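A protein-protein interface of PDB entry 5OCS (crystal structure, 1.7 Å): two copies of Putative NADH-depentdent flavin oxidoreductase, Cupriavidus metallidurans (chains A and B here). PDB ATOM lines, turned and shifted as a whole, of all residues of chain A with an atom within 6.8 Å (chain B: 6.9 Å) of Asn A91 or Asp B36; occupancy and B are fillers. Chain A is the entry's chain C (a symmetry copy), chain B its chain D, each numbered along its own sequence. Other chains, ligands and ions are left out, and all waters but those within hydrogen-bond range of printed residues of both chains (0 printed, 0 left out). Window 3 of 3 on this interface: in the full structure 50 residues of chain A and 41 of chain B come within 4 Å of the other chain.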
ATOM      1  N   MET A  39     -21.966  31.279 -19.998  1.00  0.00           N
ATOM      2  CA  MET A  39     -22.959  30.841 -19.017  1.00  0.00           C
ATOM      3  C   MET A  39     -22.378  30.928 -17.591  1.00  0.00           C
ATOM      4  O   MET A  39     -23.054  31.412 -16.692  1.00  0.00           O
ATOM      5  CB  MET A  39     -23.525  29.448 -19.246  1.00  0.00           C
ATOM      6  CG  MET A  39     -24.924  29.298 -18.515  1.00  0.00           C
ATOM      7  SD  MET A  39     -25.513  27.685 -18.737  1.00  0.00           S
ATOM      8  CE  MET A  39     -26.102  27.915 -20.409  1.00  0.00           C
ATOM      9  N   ARG A  84     -29.204  30.874 -25.190  1.00  0.00           N
ATOM     10  CA  ARG A  84     -28.991  29.789 -24.201  1.00  0.00           C
ATOM     11  C   ARG A  84     -28.486  30.357 -22.890  1.00  0.00           C
ATOM     12  O   ARG A  84     -28.972  29.993 -21.810  1.00  0.00           O
ATOM     13  CB  ARG A  84     -28.053  28.714 -24.724  1.00  0.00           C
ATOM     14  CG  ARG A  84     -28.716  27.746 -25.706  1.00  0.00           C
ATOM     15  CD  ARG A  84     -27.757  26.630 -26.121  1.00  0.00           C
ATOM     16  NE  ARG A  84     -26.788  27.081 -27.139  1.00  0.00           N
ATOM     17  CZ  ARG A  84     -27.053  27.274 -28.450  1.00  0.00           C
ATOM     18  NH1 ARG A  84     -28.271  27.057 -28.960  1.00  0.00           N
ATOM     19  NH2 ARG A  84     -26.093  27.685 -29.272  1.00  0.00           N
ATOM     20  N   VAL A  85     -27.548  31.299 -22.991  1.00  0.00           N
ATOM     21  CA  VAL A  85     -26.992  31.889 -21.801  1.00  0.00           C
ATOM     22  C   VAL A  85     -28.040  32.671 -21.029  1.00  0.00           C
ATOM     23  O   VAL A  85     -28.195  32.535 -19.826  1.00  0.00           O
ATOM     24  CB  VAL A  85     -25.786  32.782 -22.131  1.00  0.00           C
ATOM     25  CG1 VAL A  85     -25.268  33.406 -20.847  1.00  0.00           C
ATOM     26  CG2 VAL A  85     -24.694  31.964 -22.775  1.00  0.00           C
ATOM     27  N   LEU A  86     -28.786  33.497 -21.765  1.00  0.00           N
ATOM     28  CA  LEU A  86     -29.821  34.339 -21.190  1.00  0.00           C
ATOM     29  C   LEU A  86     -30.918  33.517 -20.502  1.00  0.00           C
ATOM     30  O   LEU A  86     -31.355  33.901 -19.438  1.00  0.00           O
ATOM     31  CB  LEU A  86     -30.448  35.205 -22.264  1.00  0.00           C
ATOM     32  CG  LEU A  86     -29.576  36.306 -22.810  1.00  0.00           C
ATOM     33  CD1 LEU A  86     -30.380  37.003 -23.915  1.00  0.00           C
ATOM     34  CD2 LEU A  86     -29.159  37.258 -21.708  1.00  0.00           C
ATOM     35  N   GLY A  87     -31.257  32.364 -21.058  1.00  0.00           N
ATOM     36  CA  GLY A  87     -32.246  31.470 -20.428  1.00  0.00           C
ATOM     37  C   GLY A  87     -31.811  31.044 -19.038  1.00  0.00           C
ATOM     38  O   GLY A  87     -32.579  31.105 -18.082  1.00  0.00           O
ATOM     39  N   ALA A  88     -30.535  30.701 -18.926  1.00  0.00           N
ATOM     40  CA  ALA A  88     -29.943  30.323 -17.634  1.00  0.00           C
ATOM     41  C   ALA A  88     -29.956  31.477 -16.658  1.00  0.00           C
ATOM     42  O   ALA A  88     -30.263  31.310 -15.470  1.00  0.00           O
ATOM     43  CB  ALA A  88     -28.520  29.804 -17.807  1.00  0.00           C
ATOM     44  N   VAL A  89     -29.564  32.664 -17.133  1.00  0.00           N
ATOM     45  CA  VAL A  89     -29.566  33.845 -16.302  1.00  0.00           C
ATOM     46  C   VAL A  89     -30.976  34.140 -15.787  1.00  0.00           C
ATOM     47  O   VAL A  89     -31.178  34.353 -14.604  1.00  0.00           O
ATOM     48  CB  VAL A  89     -28.999  35.064 -17.092  1.00  0.00           C
ATOM     49  CG1 VAL A  89     -29.274  36.379 -16.414  1.00  0.00           C
ATOM     50  CG2 VAL A  89     -27.514  34.876 -17.330  1.00  0.00           C
ATOM     51  N   ARG A  90     -31.954  34.183 -16.678  1.00  0.00           N
ATOM     52  CA  ARG A  90     -33.339  34.476 -16.264  1.00  0.00           C
ATOM     53  C   ARG A  90     -33.896  33.420 -15.276  1.00  0.00           C
ATOM     54  O   ARG A  90     -34.690  33.767 -14.395  1.00  0.00           O
ATOM     55  CB  ARG A  90     -34.293  34.578 -17.477  1.00  0.00           C
ATOM     56  CG  ARG A  90     -34.441  35.953 -18.115  1.00  0.00           C
ATOM     57  CD  ARG A  90     -33.143  36.594 -18.519  1.00  0.00           C
ATOM     58  NE  ARG A  90     -33.413  37.749 -19.415  1.00  0.00           N
ATOM     59  CZ  ARG A  90     -33.634  39.014 -19.044  1.00  0.00           C
ATOM     60  NH1 ARG A  90     -33.644  39.394 -17.769  1.00  0.00           N
ATOM     61  NH2 ARG A  90     -33.851  39.944 -19.981  1.00  0.00           N
ATOM     62  N   ASN A  91     -33.465  32.171 -15.426  1.00  0.00           N
ATOM     63  CA  ASN A  91     -33.852  31.087 -14.499  1.00  0.00           C
ATOM     64  C   ASN A  91     -33.360  31.293 -13.083  1.00  0.00           C
ATOM     65  O   ASN A  91     -33.927  30.726 -12.160  1.00  0.00           O
ATOM     66  CB  ASN A  91     -33.366  29.732 -14.979  1.00  0.00           C
ATOM     67  CG  ASN A  91     -34.225  29.136 -16.073  1.00  0.00           C
ATOM     68  OD1 ASN A  91     -35.405  29.498 -16.269  1.00  0.00           O
ATOM     69  ND2 ASN A  91     -33.647  28.181 -16.774  1.00  0.00           N
ATOM     70  N   HIS A  92     -32.283  32.040 -12.904  1.00  0.00           N
ATOM     71  CA  HIS A  92     -31.685  32.205 -11.573  1.00  0.00           C
ATOM     72  C   HIS A  92     -31.566  33.625 -11.055  1.00  0.00           C
ATOM     73  O   HIS A  92     -31.001  33.820  -9.994  1.00  0.00           O
ATOM     74  CB  HIS A  92     -30.344  31.463 -11.527  1.00  0.00           C
ATOM     75  CG  HIS A  92     -30.498  30.013 -11.801  1.00  0.00           C
ATOM     76  ND1 HIS A  92     -31.051  29.152 -10.875  1.00  0.00           N
ATOM     77  CD2 HIS A  92     -30.254  29.277 -12.911  1.00  0.00           C
ATOM     78  CE1 HIS A  92     -31.141  27.949 -11.400  1.00  0.00           C
ATOM     79  NE2 HIS A  92     -30.647  27.992 -12.628  1.00  0.00           N
ATOM     80  N   SER A  93     -32.097  34.619 -11.770  1.00  0.00           N
ATOM     81  CA  SER A  93     -31.948  35.980 -11.334  1.00  0.00           C
ATOM     82  C   SER A  93     -32.994  36.912 -11.913  1.00  0.00           C
ATOM     83  O   SER A  93     -33.402  36.738 -13.058  1.00  0.00           O
ATOM     84  CB  SER A  93     -30.570  36.488 -11.779  1.00  0.00           C
ATOM     85  OG  SER A  93     -30.393  37.848 -11.514  1.00  0.00           O
ATOM     86  N   SER B  28     -30.668  21.276  -6.547  1.00  0.00           N
ATOM     87  CA  SER B  28     -30.997  21.931  -7.825  1.00  0.00           C
ATOM     88  C   SER B  28     -30.944  20.982  -9.028  1.00  0.00           C
ATOM     89  O   SER B  28     -30.721  21.418 -10.164  1.00  0.00           O
ATOM     90  CB  SER B  28     -30.019  23.105  -8.037  1.00  0.00           C
ATOM     91  OG  SER B  28     -30.243  24.096  -7.065  1.00  0.00           O
ATOM     92  N   ASN B  33     -30.408  14.671 -12.315  1.00  0.00           N
ATOM     93  CA  ASN B  33     -29.666  15.344 -13.359  1.00  0.00           C
ATOM     94  C   ASN B  33     -29.220  16.764 -13.017  1.00  0.00           C
ATOM     95  O   ASN B  33     -30.034  17.621 -12.654  1.00  0.00           O
ATOM     96  CB  ASN B  33     -30.508  15.429 -14.650  1.00  0.00           C
ATOM     97  CG  ASN B  33     -30.890  14.082 -15.191  1.00  0.00           C
ATOM     98  OD1 ASN B  33     -30.105  13.162 -15.225  1.00  0.00           O
ATOM     99  ND2 ASN B  33     -32.110  13.975 -15.633  1.00  0.00           N
ATOM    100  N   ALA B  34     -27.936  17.018 -13.198  1.00  0.00           N
ATOM    101  CA  ALA B  34     -27.417  18.357 -13.099  1.00  0.00           C
ATOM    102  C   ALA B  34     -28.136  19.266 -14.071  1.00  0.00           C
ATOM    103  O   ALA B  34     -28.547  18.845 -15.161  1.00  0.00           O
ATOM    104  CB  ALA B  34     -25.914  18.386 -13.362  1.00  0.00           C
ATOM    105  N   THR B  35     -28.275  20.517 -13.667  1.00  0.00           N
ATOM    106  CA  THR B  35     -28.987  21.548 -14.443  1.00  0.00           C
ATOM    107  C   THR B  35     -28.049  22.699 -14.746  1.00  0.00           C
ATOM    108  O   THR B  35     -26.872  22.666 -14.399  1.00  0.00           O
ATOM    109  CB  THR B  35     -30.217  22.066 -13.682  1.00  0.00           C
ATOM    110  OG1 THR B  35     -29.784  22.730 -12.472  1.00  0.00           O
ATOM    111  CG2 THR B  35     -31.132  20.919 -13.308  1.00  0.00           C
ATOM    112  N   ASP B  36     -28.584  23.730 -15.367  1.00  0.00           N
ATOM    113  CA  ASP B  36     -27.794  24.917 -15.652  1.00  0.00           C
ATOM    114  C   ASP B  36     -27.211  25.523 -14.380  1.00  0.00           C
ATOM    115  O   ASP B  36     -26.115  26.093 -14.411  1.00  0.00           O
ATOM    116  CB  ASP B  36     -28.583  25.974 -16.452  1.00  0.00           C
ATOM    117  CG  ASP B  36     -29.941  26.423 -15.810  1.00  0.00           C
ATOM    118  OD1 ASP B  36     -30.311  26.087 -14.627  1.00  0.00           O
ATOM    119  OD2 ASP B  36     -30.703  27.167 -16.533  1.00  0.00           O
ATOM    120  N   TRP B  37     -27.900  25.353 -13.257  1.00  0.00           N
ATOM    121  CA  TRP B  37     -27.366  25.844 -11.983  1.00  0.00           C
ATOM    122  C   TRP B  37     -25.985  25.249 -11.710  1.00  0.00           C
ATOM    123  O   TRP B  37     -25.078  25.962 -11.252  1.00  0.00           O
ATOM    124  CB  TRP B  37     -28.291  25.497 -10.816  1.00  0.00           C
ATOM    125  CG  TRP B  37     -27.678  25.915  -9.509  1.00  0.00           C
ATOM    126  CD1 TRP B  37     -27.065  25.115  -8.596  1.00  0.00           C
ATOM    127  CD2 TRP B  37     -27.483  27.246  -9.065  1.00  0.00           C
ATOM    128  NE1 TRP B  37     -26.559  25.863  -7.581  1.00  0.00           N
ATOM    129  CE2 TRP B  37     -26.795  27.183  -7.846  1.00  0.00           C
ATOM    130  CE3 TRP B  37     -27.849  28.490  -9.561  1.00  0.00           C
ATOM    131  CZ2 TRP B  37     -26.479  28.300  -7.128  1.00  0.00           C
ATOM    132  CZ3 TRP B  37     -27.548  29.610  -8.817  1.00  0.00           C
ATOM    133  CH2 TRP B  37     -26.864  29.512  -7.626  1.00  0.00           C
ATOM    134  N   HIS B  38     -25.828  23.943 -11.924  1.00  0.00           N
ATOM    135  CA  HIS B  38     -24.569  23.286 -11.622  1.00  0.00           C
ATOM    136  C   HIS B  38     -23.450  23.794 -12.491  1.00  0.00           C
ATOM    137  O   HIS B  38     -22.323  23.935 -12.017  1.00  0.00           O
ATOM    138  CB  HIS B  38     -24.651  21.779 -11.713  1.00  0.00           C
ATOM    139  CG  HIS B  38     -25.531  21.192 -10.669  1.00  0.00           C
ATOM    140  ND1 HIS B  38     -26.873  21.031 -10.851  1.00  0.00           N
ATOM    141  CD2 HIS B  38     -25.274  20.804  -9.405  1.00  0.00           C
ATOM    142  CE1 HIS B  38     -27.417  20.554  -9.742  1.00  0.00           C
ATOM    143  NE2 HIS B  38     -26.453  20.380  -8.861  1.00  0.00           N
ATOM    144  N   MET B  39     -23.733  24.082 -13.749  1.00  0.00           N
ATOM    145  CA  MET B  39     -22.767  24.764 -14.621  1.00  0.00           C
ATOM    146  C   MET B  39     -22.269  26.080 -14.013  1.00  0.00           C
ATOM    147  O   MET B  39     -21.068  26.346 -13.916  1.00  0.00           O
ATOM    148  CB  MET B  39     -23.430  25.039 -15.991  1.00  0.00           C
ATOM    149  CG  MET B  39     -22.542  25.753 -16.996  1.00  0.00           C
ATOM    150  SD  MET B  39     -21.151  24.737 -17.510  1.00  0.00           S
ATOM    151  CE  MET B  39     -21.988  23.546 -18.569  1.00  0.00           C
ATOM    152  N   ILE B  40     -23.210  26.929 -13.641  1.00  0.00           N
ATOM    153  CA  ILE B  40     -22.886  28.261 -13.070  1.00  0.00           C
ATOM    154  C   ILE B  40     -22.153  28.145 -11.724  1.00  0.00           C
ATOM    155  O   ILE B  40     -21.088  28.769 -11.489  1.00  0.00           O
ATOM    156  CB  ILE B  40     -24.188  29.082 -12.864  1.00  0.00           C
ATOM    157  CG1 ILE B  40     -24.865  29.302 -14.229  1.00  0.00           C
ATOM    158  CG2 ILE B  40     -23.870  30.399 -12.158  1.00  0.00           C
ATOM    159  CD1 ILE B  40     -26.270  29.892 -14.230  1.00  0.00           C
ATOM    160  N   HIS B  41     -22.657  27.272 -10.878  1.00  0.00           N
ATOM    161  CA  HIS B  41     -22.098  27.092  -9.526  1.00  0.00           C
ATOM    162  C   HIS B  41     -20.767  26.397  -9.490  1.00  0.00           C
ATOM    163  O   HIS B  41     -19.790  26.907  -8.902  1.00  0.00           O
ATOM    164  CB  HIS B  41     -23.131  26.342  -8.689  1.00  0.00           C
ATOM    165  CG  HIS B  41     -22.639  25.950  -7.338  1.00  0.00           C
ATOM    166  ND1 HIS B  41     -22.345  26.869  -6.357  1.00  0.00           N
ATOM    167  CD2 HIS B  41     -22.341  24.735  -6.828  1.00  0.00           C
ATOM    168  CE1 HIS B  41     -21.931  26.229  -5.281  1.00  0.00           C
ATOM    169  NE2 HIS B  41     -21.889  24.939  -5.553  1.00  0.00           N
ATOM    170  N   VAL B  85     -21.384  19.565 -17.436  1.00  0.00           N
ATOM    171  CA  VAL B  85     -20.796  20.500 -16.467  1.00  0.00           C
ATOM    172  C   VAL B  85     -19.298  20.306 -16.362  1.00  0.00           C
ATOM    173  O   VAL B  85     -18.519  21.281 -16.432  1.00  0.00           O
ATOM    174  CB  VAL B  85     -21.443  20.343 -15.072  1.00  0.00           C
ATOM    175  CG1 VAL B  85     -20.789  21.279 -14.076  1.00  0.00           C
ATOM    176  CG2 VAL B  85     -22.924  20.681 -15.134  1.00  0.00           C
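The side-chain amide nitrogen (ND2) of Asn A91 lies close to the backbone carbonyl oxygen (O) of Gly A87 (3.4 Å). The backbone NH of Trp B37 sits close to the side-chain hydroxyl of Thr B35 (3.3 Å).
Met A39 touches Met B39. O of Met A39 touches CG1 of Ile B40, 3.7 Å away. Ala A88 touches Asp B36 (CA to OD2, 3.4 Å). CE3 of Trp B37 touches ND1 of His A92 (3.5 Å).
Met A39 touches its own counterpart, Met B39. Positions printed for both chains: 39 and 85.
NE2 of His A92 sits at hydrogen-bond distance from OD1 of Asp B36. The side-chain amide nitrogen (ND2) of Asn A91 is in hydrogen-bond range of the side-chain carboxylate (OD2) of Asp B36, at 3.1 Å.
Of the 11 printed residues of chain A, 4 touch a printed residue of chain B. Hydrophobic or aromatic side chains of chain A that line the printed part of chain B: Met A39, Ala A88 and His A92. Hydrophobic or aromatic side chains of chain B that line the printed part of chain A: Trp B37, Met B39 and Ile B40. Among the printed residues, 6 pairs touch across the chains.
Of the printed residues of chain B, Met A39 touches Met B39 (3.9 Å) and Ile B40 (3.7 Å). Arg A90 touches none of the printed residues of chain B. Ala B34 touches none of the printed residues of chain A. Asp B36 touches just these residues of chain A: Ala A88, Asn A91 and His A92. Of the printed residues of chain A, Trp B37 touches His A92. Printed residues of chain A within 4 Å of Ile B40: Met A39 (3.7 Å). The nearest printed residue of chain B that does not touch Asn A91 is Trp B37 (7.0 Å). The nearest residue of chain A that does not touch Asp B36 is Met A39 (4.2 Å). The nearest printed residue of chain B that does not touch Ala A88 is Ile B40 (4.2 Å).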
